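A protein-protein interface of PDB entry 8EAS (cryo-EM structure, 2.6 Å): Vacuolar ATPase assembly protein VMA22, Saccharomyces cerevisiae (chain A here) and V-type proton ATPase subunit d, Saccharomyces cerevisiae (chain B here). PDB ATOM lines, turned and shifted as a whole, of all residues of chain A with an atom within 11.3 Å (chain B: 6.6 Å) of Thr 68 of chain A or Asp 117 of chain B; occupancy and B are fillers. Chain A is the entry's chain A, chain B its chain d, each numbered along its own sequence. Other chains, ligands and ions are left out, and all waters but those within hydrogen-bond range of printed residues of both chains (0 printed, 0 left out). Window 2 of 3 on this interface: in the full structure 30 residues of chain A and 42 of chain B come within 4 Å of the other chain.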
ATOM      1  N   GLU A  62     -17.523  18.825  20.396  1.00  0.00           N
ATOM      2  CA  GLU A  62     -18.517  19.419  21.286  1.00  0.00           C
ATOM      3  C   GLU A  62     -18.166  19.237  22.756  1.00  0.00           C
ATOM      4  O   GLU A  62     -18.671  19.975  23.606  1.00  0.00           O
ATOM      5  CB  GLU A  62     -19.892  18.824  20.996  1.00  0.00           C
ATOM      6  CG  GLU A  62     -19.998  17.346  21.312  1.00  0.00           C
ATOM      7  CD  GLU A  62     -21.350  16.774  20.953  1.00  0.00           C
ATOM      8  OE1 GLU A  62     -22.194  17.535  20.436  1.00  0.00           O
ATOM      9  OE2 GLU A  62     -21.567  15.568  21.186  1.00  0.00           O
ATOM     10  N   ASP A  63     -17.318  18.262  23.080  1.00  0.00           N
ATOM     11  CA  ASP A  63     -16.901  18.078  24.463  1.00  0.00           C
ATOM     12  C   ASP A  63     -16.169  19.298  24.992  1.00  0.00           C
ATOM     13  O   ASP A  63     -16.179  19.558  26.200  1.00  0.00           O
ATOM     14  CB  ASP A  63     -16.007  16.849  24.575  1.00  0.00           C
ATOM     15  CG  ASP A  63     -16.772  15.563  24.412  1.00  0.00           C
ATOM     16  OD1 ASP A  63     -16.198  14.601  23.865  1.00  0.00           O
ATOM     17  OD2 ASP A  63     -17.944  15.513  24.835  1.00  0.00           O
ATOM     18  N   TYR A  64     -15.533  20.055  24.105  1.00  0.00           N
ATOM     19  CA  TYR A  64     -14.703  21.183  24.482  1.00  0.00           C
ATOM     20  C   TYR A  64     -15.332  22.527  24.167  1.00  0.00           C
ATOM     21  O   TYR A  64     -14.728  23.556  24.481  1.00  0.00           O
ATOM     22  CB  TYR A  64     -13.357  21.104  23.763  1.00  0.00           C
ATOM     23  CG  TYR A  64     -12.505  19.929  24.149  1.00  0.00           C
ATOM     24  CD1 TYR A  64     -11.799  19.917  25.338  1.00  0.00           C
ATOM     25  CD2 TYR A  64     -12.401  18.830  23.317  1.00  0.00           C
ATOM     26  CE1 TYR A  64     -11.015  18.856  25.677  1.00  0.00           C
ATOM     27  CE2 TYR A  64     -11.620  17.762  23.652  1.00  0.00           C
ATOM     28  CZ  TYR A  64     -10.930  17.778  24.835  1.00  0.00           C
ATOM     29  OH  TYR A  64     -10.148  16.710  25.182  1.00  0.00           O
ATOM     30  N   TRP A  65     -16.497  22.551  23.535  1.00  0.00           N
ATOM     31  CA  TRP A  65     -17.087  23.815  23.126  1.00  0.00           C
ATOM     32  C   TRP A  65     -17.462  24.636  24.344  1.00  0.00           C
ATOM     33  O   TRP A  65     -18.211  24.180  25.212  1.00  0.00           O
ATOM     34  CB  TRP A  65     -18.311  23.572  22.258  1.00  0.00           C
ATOM     35  CG  TRP A  65     -17.982  23.004  20.939  1.00  0.00           C
ATOM     36  CD1 TRP A  65     -16.745  22.857  20.394  1.00  0.00           C
ATOM     37  CD2 TRP A  65     -18.906  22.509  19.979  1.00  0.00           C
ATOM     38  NE1 TRP A  65     -16.841  22.288  19.153  1.00  0.00           N
ATOM     39  CE2 TRP A  65     -18.162  22.066  18.876  1.00  0.00           C
ATOM     40  CE3 TRP A  65     -20.295  22.384  19.949  1.00  0.00           C
ATOM     41  CZ2 TRP A  65     -18.759  21.513  17.755  1.00  0.00           C
ATOM     42  CZ3 TRP A  65     -20.882  21.838  18.840  1.00  0.00           C
ATOM     43  CH2 TRP A  65     -20.119  21.409  17.755  1.00  0.00           C
ATOM     44  N   ASP A  66     -16.943  25.853  24.397  1.00  0.00           N
ATOM     45  CA  ASP A  66     -17.174  26.768  25.504  1.00  0.00           C
ATOM     46  C   ASP A  66     -18.340  27.649  25.077  1.00  0.00           C
ATOM     47  O   ASP A  66     -18.191  28.524  24.225  1.00  0.00           O
ATOM     48  CB  ASP A  66     -15.900  27.558  25.789  1.00  0.00           C
ATOM     49  CG  ASP A  66     -16.113  28.743  26.712  1.00  0.00           C
ATOM     50  OD1 ASP A  66     -15.133  29.482  26.924  1.00  0.00           O
ATOM     51  OD2 ASP A  66     -17.209  28.914  27.276  1.00  0.00           O
ATOM     52  N   GLU A  67     -19.517  27.401  25.648  1.00  0.00           N
ATOM     53  CA  GLU A  67     -20.692  28.183  25.286  1.00  0.00           C
ATOM     54  C   GLU A  67     -20.652  29.596  25.840  1.00  0.00           C
ATOM     55  O   GLU A  67     -21.495  30.413  25.463  1.00  0.00           O
ATOM     56  CB  GLU A  67     -21.959  27.475  25.753  1.00  0.00           C
ATOM     57  CG  GLU A  67     -22.593  26.620  24.680  1.00  0.00           C
ATOM     58  CD  GLU A  67     -21.894  25.297  24.521  1.00  0.00           C
ATOM     59  OE1 GLU A  67     -21.182  24.895  25.459  1.00  0.00           O
ATOM     60  OE2 GLU A  67     -22.056  24.657  23.461  1.00  0.00           O
ATOM     61  N   THR A  68     -19.708  29.899  26.718  1.00  0.00           N
ATOM     62  CA  THR A  68     -19.474  31.261  27.169  1.00  0.00           C
ATOM     63  C   THR A  68     -18.379  31.949  26.372  1.00  0.00           C
ATOM     64  O   THR A  68     -17.961  33.049  26.738  1.00  0.00           O
ATOM     65  CB  THR A  68     -19.120  31.269  28.655  1.00  0.00           C
ATOM     66  OG1 THR A  68     -17.919  30.520  28.865  1.00  0.00           O
ATOM     67  CG2 THR A  68     -20.236  30.647  29.456  1.00  0.00           C
ATOM     68  N   TYR A  69     -17.910  31.328  25.295  1.00  0.00           N
ATOM     69  CA  TYR A  69     -16.770  31.844  24.553  1.00  0.00           C
ATOM     70  C   TYR A  69     -17.214  32.978  23.643  1.00  0.00           C
ATOM     71  O   TYR A  69     -18.015  32.771  22.726  1.00  0.00           O
ATOM     72  CB  TYR A  69     -16.116  30.734  23.734  1.00  0.00           C
ATOM     73  CG  TYR A  69     -14.981  31.218  22.869  1.00  0.00           C
ATOM     74  CD1 TYR A  69     -13.868  31.815  23.432  1.00  0.00           C
ATOM     75  CD2 TYR A  69     -15.028  31.092  21.490  1.00  0.00           C
ATOM     76  CE1 TYR A  69     -12.834  32.264  22.654  1.00  0.00           C
ATOM     77  CE2 TYR A  69     -13.994  31.543  20.702  1.00  0.00           C
ATOM     78  CZ  TYR A  69     -12.901  32.127  21.291  1.00  0.00           C
ATOM     79  OH  TYR A  69     -11.860  32.583  20.523  1.00  0.00           O
ATOM     80  N   ILE A  70     -16.699  34.171  23.896  1.00  0.00           N
ATOM     81  CA  ILE A  70     -16.803  35.274  22.951  1.00  0.00           C
ATOM     82  C   ILE A  70     -15.557  35.243  22.078  1.00  0.00           C
ATOM     83  O   ILE A  70     -14.438  35.076  22.576  1.00  0.00           O
ATOM     84  CB  ILE A  70     -16.956  36.621  23.677  1.00  0.00           C
ATOM     85  CG1 ILE A  70     -15.777  36.877  24.613  1.00  0.00           C
ATOM     86  CG2 ILE A  70     -18.256  36.652  24.454  1.00  0.00           C
ATOM     87  CD1 ILE A  70     -15.732  38.281  25.153  1.00  0.00           C
ATOM     88  N   GLY A  71     -15.748  35.373  20.781  1.00  0.00           N
ATOM     89  CA  GLY A  71     -14.686  35.071  19.854  1.00  0.00           C
ATOM     90  C   GLY A  71     -13.592  36.114  19.827  1.00  0.00           C
ATOM     91  O   GLY A  71     -13.627  37.141  20.502  1.00  0.00           O
ATOM     92  N   GLN A  72     -12.580  35.812  19.024  1.00  0.00           N
ATOM     93  CA  GLN A  72     -11.513  36.752  18.737  1.00  0.00           C
ATOM     94  C   GLN A  72     -11.826  37.648  17.550  1.00  0.00           C
ATOM     95  O   GLN A  72     -11.035  38.548  17.253  1.00  0.00           O
ATOM     96  CB  GLN A  72     -10.218  35.988  18.468  1.00  0.00           C
ATOM     97  CG  GLN A  72      -9.718  35.197  19.648  1.00  0.00           C
ATOM     98  CD  GLN A  72      -8.267  34.826  19.509  1.00  0.00           C
ATOM     99  OE1 GLN A  72      -7.460  35.076  20.402  1.00  0.00           O
ATOM    100  NE2 GLN A  72      -7.920  34.223  18.380  1.00  0.00           N
ATOM    101  N   LYS A  92     -13.163  41.933  19.546  1.00  0.00           N
ATOM    102  CA  LYS A  92     -14.424  41.471  20.126  1.00  0.00           C
ATOM    103  C   LYS A  92     -14.674  39.985  19.896  1.00  0.00           C
ATOM    104  O   LYS A  92     -15.801  39.510  20.031  1.00  0.00           O
ATOM    105  CB  LYS A  92     -15.596  42.278  19.568  1.00  0.00           C
ATOM    106  N   LYS A 127      -9.465  35.865  31.729  1.00  0.00           N
ATOM    107  CA  LYS A 127      -9.250  36.544  30.456  1.00  0.00           C
ATOM    108  C   LYS A 127     -10.182  36.004  29.377  1.00  0.00           C
ATOM    109  O   LYS A 127     -10.152  34.816  29.059  1.00  0.00           O
ATOM    110  CB  LYS A 127      -7.795  36.396  30.010  1.00  0.00           C
ATOM    111  N   GLN A 128     -11.006  36.882  28.812  1.00  0.00           N
ATOM    112  CA  GLN A 128     -11.918  36.495  27.744  1.00  0.00           C
ATOM    113  C   GLN A 128     -11.154  36.446  26.423  1.00  0.00           C
ATOM    114  O   GLN A 128      -9.921  36.456  26.402  1.00  0.00           O
ATOM    115  CB  GLN A 128     -13.112  37.444  27.696  1.00  0.00           C
ATOM    116  CG  GLN A 128     -13.906  37.485  28.990  1.00  0.00           C
ATOM    117  CD  GLN A 128     -14.369  36.109  29.437  1.00  0.00           C
ATOM    118  OE1 GLN A 128     -14.656  35.238  28.617  1.00  0.00           O
ATOM    119  NE2 GLN A 128     -14.432  35.908  30.747  1.00  0.00           N
ATOM    120  N   ASP A 129     -11.897  36.321  25.315  1.00  0.00           N
ATOM    121  CA  ASP A 129     -11.433  36.293  23.924  1.00  0.00           C
ATOM    122  C   ASP A 129     -10.061  35.646  23.780  1.00  0.00           C
ATOM    123  O   ASP A 129      -9.172  36.188  23.117  1.00  0.00           O
ATOM    124  CB  ASP A 129     -11.467  37.691  23.268  1.00  0.00           C
ATOM    125  CG  ASP A 129     -10.536  38.722  23.911  1.00  0.00           C
ATOM    126  OD1 ASP A 129      -9.847  38.449  24.904  1.00  0.00           O
ATOM    127  OD2 ASP A 129     -10.496  39.854  23.388  1.00  0.00           O
ATOM    128  N   TYR A 130      -9.890  34.477  24.387  1.00  0.00           N
ATOM    129  CA  TYR A 130      -8.604  33.804  24.414  1.00  0.00           C
ATOM    130  C   TYR A 130      -8.353  33.062  23.104  1.00  0.00           C
ATOM    131  O   TYR A 130      -9.190  33.032  22.199  1.00  0.00           O
ATOM    132  CB  TYR A 130      -8.543  32.836  25.593  1.00  0.00           C
ATOM    133  CG  TYR A 130      -9.719  31.887  25.666  1.00  0.00           C
ATOM    134  CD1 TYR A 130     -10.871  32.230  26.355  1.00  0.00           C
ATOM    135  CD2 TYR A 130      -9.672  30.646  25.057  1.00  0.00           C
ATOM    136  CE1 TYR A 130     -11.944  31.365  26.423  1.00  0.00           C
ATOM    137  CE2 TYR A 130     -10.735  29.779  25.122  1.00  0.00           C
ATOM    138  CZ  TYR A 130     -11.868  30.141  25.806  1.00  0.00           C
ATOM    139  OH  TYR A 130     -12.929  29.274  25.871  1.00  0.00           O
ATOM    140  N   PRO A 132      -8.523  30.173  20.791  1.00  0.00           N
ATOM    141  CA  PRO A 132      -9.533  29.105  20.820  1.00  0.00           C
ATOM    142  C   PRO A 132      -8.964  27.723  21.042  1.00  0.00           C
ATOM    143  O   PRO A 132      -9.722  26.809  21.379  1.00  0.00           O
ATOM    144  CB  PRO A 132     -10.188  29.210  19.442  1.00  0.00           C
ATOM    145  CG  PRO A 132      -9.960  30.590  19.021  1.00  0.00           C
ATOM    146  CD  PRO A 132      -8.637  30.994  19.576  1.00  0.00           C
ATOM    147  N   LEU A 134      -7.314  26.842  23.444  1.00  0.00           N
ATOM    148  CA  LEU A 134      -7.427  26.564  24.872  1.00  0.00           C
ATOM    149  C   LEU A 134      -8.793  26.002  25.232  1.00  0.00           C
ATOM    150  O   LEU A 134      -8.943  25.371  26.284  1.00  0.00           O
ATOM    151  CB  LEU A 134      -7.146  27.828  25.680  1.00  0.00           C
ATOM    152  CG  LEU A 134      -5.896  28.625  25.308  1.00  0.00           C
ATOM    153  CD1 LEU A 134      -5.844  29.924  26.094  1.00  0.00           C
ATOM    154  CD2 LEU A 134      -4.641  27.807  25.529  1.00  0.00           C
ATOM    155  N   MET A 135      -9.800  26.228  24.386  1.00  0.00           N
ATOM    156  CA  MET A 135     -11.089  25.567  24.563  1.00  0.00           C
ATOM    157  C   MET A 135     -10.928  24.059  24.624  1.00  0.00           C
ATOM    158  O   MET A 135     -11.659  23.380  25.351  1.00  0.00           O
ATOM    159  CB  MET A 135     -12.008  25.926  23.398  1.00  0.00           C
ATOM    160  CG  MET A 135     -12.430  27.365  23.316  1.00  0.00           C
ATOM    161  SD  MET A 135     -13.414  27.633  21.836  1.00  0.00           S
ATOM    162  CE  MET A 135     -14.905  26.765  22.250  1.00  0.00           C
ATOM    163  N   THR B 112     -14.851  20.280  32.593  1.00  0.00           N
ATOM    164  CA  THR B 112     -14.719  21.092  31.390  1.00  0.00           C
ATOM    165  C   THR B 112     -16.080  21.532  30.873  1.00  0.00           C
ATOM    166  O   THR B 112     -16.263  22.695  30.502  1.00  0.00           O
ATOM    167  CB  THR B 112     -13.965  20.310  30.314  1.00  0.00           C
ATOM    168  OG1 THR B 112     -12.688  19.910  30.820  1.00  0.00           O
ATOM    169  CG2 THR B 112     -13.761  21.157  29.076  1.00  0.00           C
ATOM    170  N   GLY B 113     -17.050  20.619  30.846  1.00  0.00           N
ATOM    171  CA  GLY B 113     -18.389  20.997  30.435  1.00  0.00           C
ATOM    172  C   GLY B 113     -19.042  21.968  31.398  1.00  0.00           C
ATOM    173  O   GLY B 113     -19.806  22.844  30.988  1.00  0.00           O
ATOM    174  N   THR B 114     -18.759  21.821  32.694  1.00  0.00           N
ATOM    175  CA  THR B 114     -19.347  22.714  33.683  1.00  0.00           C
ATOM    176  C   THR B 114     -18.809  24.133  33.544  1.00  0.00           C
ATOM    177  O   THR B 114     -19.581  25.097  33.516  1.00  0.00           O
ATOM    178  CB  THR B 114     -19.093  22.180  35.090  1.00  0.00           C
ATOM    179  OG1 THR B 114     -19.582  20.838  35.186  1.00  0.00           O
ATOM    180  CG2 THR B 114     -19.797  23.042  36.119  1.00  0.00           C
ATOM    181  N   ILE B 115     -17.485  24.288  33.459  1.00  0.00           N
ATOM    182  CA  ILE B 115     -16.930  25.629  33.316  1.00  0.00           C
ATOM    183  C   ILE B 115     -17.285  26.238  31.969  1.00  0.00           C
ATOM    184  O   ILE B 115     -17.272  27.465  31.826  1.00  0.00           O
ATOM    185  CB  ILE B 115     -15.402  25.639  33.513  1.00  0.00           C
ATOM    186  CG1 ILE B 115     -14.701  25.009  32.312  1.00  0.00           C
ATOM    187  CG2 ILE B 115     -15.022  24.933  34.802  1.00  0.00           C
ATOM    188  CD1 ILE B 115     -13.326  25.555  32.061  1.00  0.00           C
ATOM    189  N   HIS B 116     -17.603  25.414  30.977  1.00  0.00           N
ATOM    190  CA  HIS B 116     -18.026  25.883  29.667  1.00  0.00           C
ATOM    191  C   HIS B 116     -19.533  26.041  29.564  1.00  0.00           C
ATOM    192  O   HIS B 116     -20.031  26.400  28.493  1.00  0.00           O
ATOM    193  CB  HIS B 116     -17.533  24.923  28.585  1.00  0.00           C
ATOM    194  CG  HIS B 116     -16.053  24.969  28.367  1.00  0.00           C
ATOM    195  ND1 HIS B 116     -15.386  24.054  27.585  1.00  0.00           N
ATOM    196  CD2 HIS B 116     -15.114  25.827  28.826  1.00  0.00           C
ATOM    197  CE1 HIS B 116     -14.098  24.343  27.574  1.00  0.00           C
ATOM    198  NE2 HIS B 116     -13.906  25.416  28.318  1.00  0.00           N
ATOM    199  N   ASP B 117     -20.260  25.778  30.648  1.00  0.00           N
ATOM    200  CA  ASP B 117     -21.717  25.893  30.687  1.00  0.00           C
ATOM    201  C   ASP B 117     -22.374  25.089  29.570  1.00  0.00           C
ATOM    202  O   ASP B 117     -23.312  25.545  28.913  1.00  0.00           O
ATOM    203  CB  ASP B 117     -22.161  27.355  30.654  1.00  0.00           C
ATOM    204  CG  ASP B 117     -21.808  28.095  31.935  1.00  0.00           C
ATOM    205  OD1 ASP B 117     -21.750  27.444  32.999  1.00  0.00           O
ATOM    206  OD2 ASP B 117     -21.605  29.325  31.888  1.00  0.00           O
ATOM    207  N   ARG B 118     -21.871  23.879  29.353  1.00  0.00           N
ATOM    208  CA  ARG B 118     -22.546  22.920  28.498  1.00  0.00           C
ATOM    209  C   ARG B 118     -23.715  22.292  29.247  1.00  0.00           C
ATOM    210  O   ARG B 118     -23.776  22.307  30.479  1.00  0.00           O
ATOM    211  CB  ARG B 118     -21.579  21.832  28.037  1.00  0.00           C
ATOM    212  CG  ARG B 118     -20.664  22.258  26.915  1.00  0.00           C
ATOM    213  CD  ARG B 118     -19.775  21.125  26.443  1.00  0.00           C
ATOM    214  NE  ARG B 118     -20.498  19.871  26.282  1.00  0.00           N
ATOM    215  CZ  ARG B 118     -21.326  19.605  25.281  1.00  0.00           C
ATOM    216  NH1 ARG B 118     -21.593  20.502  24.346  1.00  0.00           N
ATOM    217  NH2 ARG B 118     -21.895  18.406  25.212  1.00  0.00           N
ATOM    218  N   ASP B 119     -24.653  21.737  28.485  1.00  0.00           N
ATOM    219  CA  ASP B 119     -25.787  21.052  29.087  1.00  0.00           C
ATOM    220  C   ASP B 119     -25.311  19.872  29.922  1.00  0.00           C
ATOM    221  O   ASP B 119     -24.472  19.083  29.479  1.00  0.00           O
ATOM    222  CB  ASP B 119     -26.755  20.576  28.008  1.00  0.00           C
ATOM    223  CG  ASP B 119     -28.017  19.966  28.584  1.00  0.00           C
ATOM    224  OD1 ASP B 119     -28.256  20.120  29.800  1.00  0.00           O
ATOM    225  OD2 ASP B 119     -28.770  19.324  27.823  1.00  0.00           O
ATOM    226  N   LYS B 120     -25.862  19.749  31.131  1.00  0.00           N
ATOM    227  CA  LYS B 120     -25.485  18.655  32.021  1.00  0.00           C
ATOM    228  C   LYS B 120     -25.804  17.300  31.403  1.00  0.00           C
ATOM    229  O   LYS B 120     -24.989  16.368  31.470  1.00  0.00           O
ATOM    230  CB  LYS B 120     -26.204  18.817  33.359  1.00  0.00           C
ATOM    231  CG  LYS B 120     -25.872  17.762  34.397  1.00  0.00           C
ATOM    232  CD  LYS B 120     -26.536  18.096  35.721  1.00  0.00           C
ATOM    233  CE  LYS B 120     -28.035  17.852  35.658  1.00  0.00           C
ATOM    234  NZ  LYS B 120     -28.696  18.060  36.975  1.00  0.00           N
ATOM    235  N   ILE B 123     -23.223  16.368  28.707  1.00  0.00           N
ATOM    236  CA  ILE B 123     -21.955  15.913  29.264  1.00  0.00           C
ATOM    237  C   ILE B 123     -22.091  14.504  29.822  1.00  0.00           C
ATOM    238  O   ILE B 123     -21.199  13.667  29.646  1.00  0.00           O
ATOM    239  CB  ILE B 123     -21.447  16.894  30.334  1.00  0.00           C
ATOM    240  CG1 ILE B 123     -21.463  18.323  29.804  1.00  0.00           C
ATOM    241  CG2 ILE B 123     -20.035  16.533  30.744  1.00  0.00           C
ATOM    242  CD1 ILE B 123     -21.546  19.351  30.892  1.00  0.00           C
ATOM    243  N   THR B 143     -17.524  24.694  40.240  1.00  0.00           N
ATOM    244  CA  THR B 143     -16.346  24.907  39.412  1.00  0.00           C
ATOM    245  C   THR B 143     -15.089  25.095  40.254  1.00  0.00           C
ATOM    246  O   THR B 143     -14.103  25.661  39.773  1.00  0.00           O
ATOM    247  CB  THR B 143     -16.552  26.108  38.489  1.00  0.00           C
ATOM    248  OG1 THR B 143     -16.858  27.268  39.271  1.00  0.00           O
ATOM    249  CG2 THR B 143     -17.688  25.845  37.513  1.00  0.00           C
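Among the printed residues, pairs that only touch across the chains: Glu 67 of chain A with Arg 118 of chain B (3.1 Å), Thr 68 of chain A with Asp 117 of chain B (3.1 Å), Met 135 of chain A with His 116 of chain B (3.4 Å), Trp 65 of chain A with His 116 of chain B (3.5 Å), Trp 65 of chain A with Arg 118 of chain B (3.6 Å), Asp 66 of chain A with His 116 of chain B (3.6 Å), Asp 63 of chain A with Arg 118 of chain B (3.9 Å), Thr 68 of chain A with His 116 of chain B (3.9 Å) and Glu 67 of chain A with Asp 117 of chain B (3.9 Å).
Printed residues of chain A that touch a printed residue of chain B: Glu 62, Asp 63, Tyr 64, Trp 65, Asp 66, Glu 67, Thr 68 and Met 135. Along chain A the printed residues that touch a printed residue of chain B span positions 62 to 135. Among the printed residues, 12 pairs touch across the chains. Among the printed residues, no Asp or Glu carboxylate lies within 4 Å of a Lys or Arg side-chain nitrogen of the other chain.
O of Thr 112 of chain B sits close to ND1 of His 116 of chain B. The side-chain hydroxyl (OH) of Tyr 130 of chain A lies within hydrogen-bond range of the side-chain carboxylate (OD1) of Asp 66 of chain A (2.5 Å). The backbone carbonyl oxygen (O) of Gly 113 of chain B lies within hydrogen-bond range of the backbone NH (N) of Arg 118 of chain B (2.8 Å). The side-chain carboxylate of Asp 66 of chain A lies within hydrogen-bond range of the backbone NH of Thr 68 of chain A (2.7 Å). The side-chain carboxylate (OD2) of Asp 66 of chain A is in hydrogen-bond range of the backbone NH (N) of Tyr 69 of chain A, 3.2 Å away.
Of the printed residues of chain B, Tyr 64 of chain A touches His 116 (3.2 Å). Of chain B, only His 116 (3.9 Å) and Asp 117 (3.1 Å) come within 4 Å of Thr 68 of chain A. Lys 127 of chain A touches none of the printed residues of chain B. Tyr 130 of chain A touches none of the printed residues of chain B. Printed residues of chain B within 4 Å of Met 135 of chain A: His 116. No residue of chain A comes within 4 Å of Gly 113 of chain B. His 116 of chain B touches just these residues of chain A: Tyr 64, Trp 65, Asp 66, Glu 67, Thr 68 and Met 135. The nearest residue of chain B that does not touch Thr 68 of chain A is Ile 115 of chain B (4.3 Å).
The backbone carbonyl oxygen (O) of His 116 of chain B is in hydrogen-bond range of the backbone NH (N) of Glu 67 of chain A, 3.1 Å away. The guanidinium group (NH1) of Arg 118 of chain B sits at hydrogen-bond distance from the backbone carbonyl oxygen (O) of Glu 62 of chain A. O of Tyr 64 of chain A sits at hydrogen-bond distance from ND1 of His 116 of chain B.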
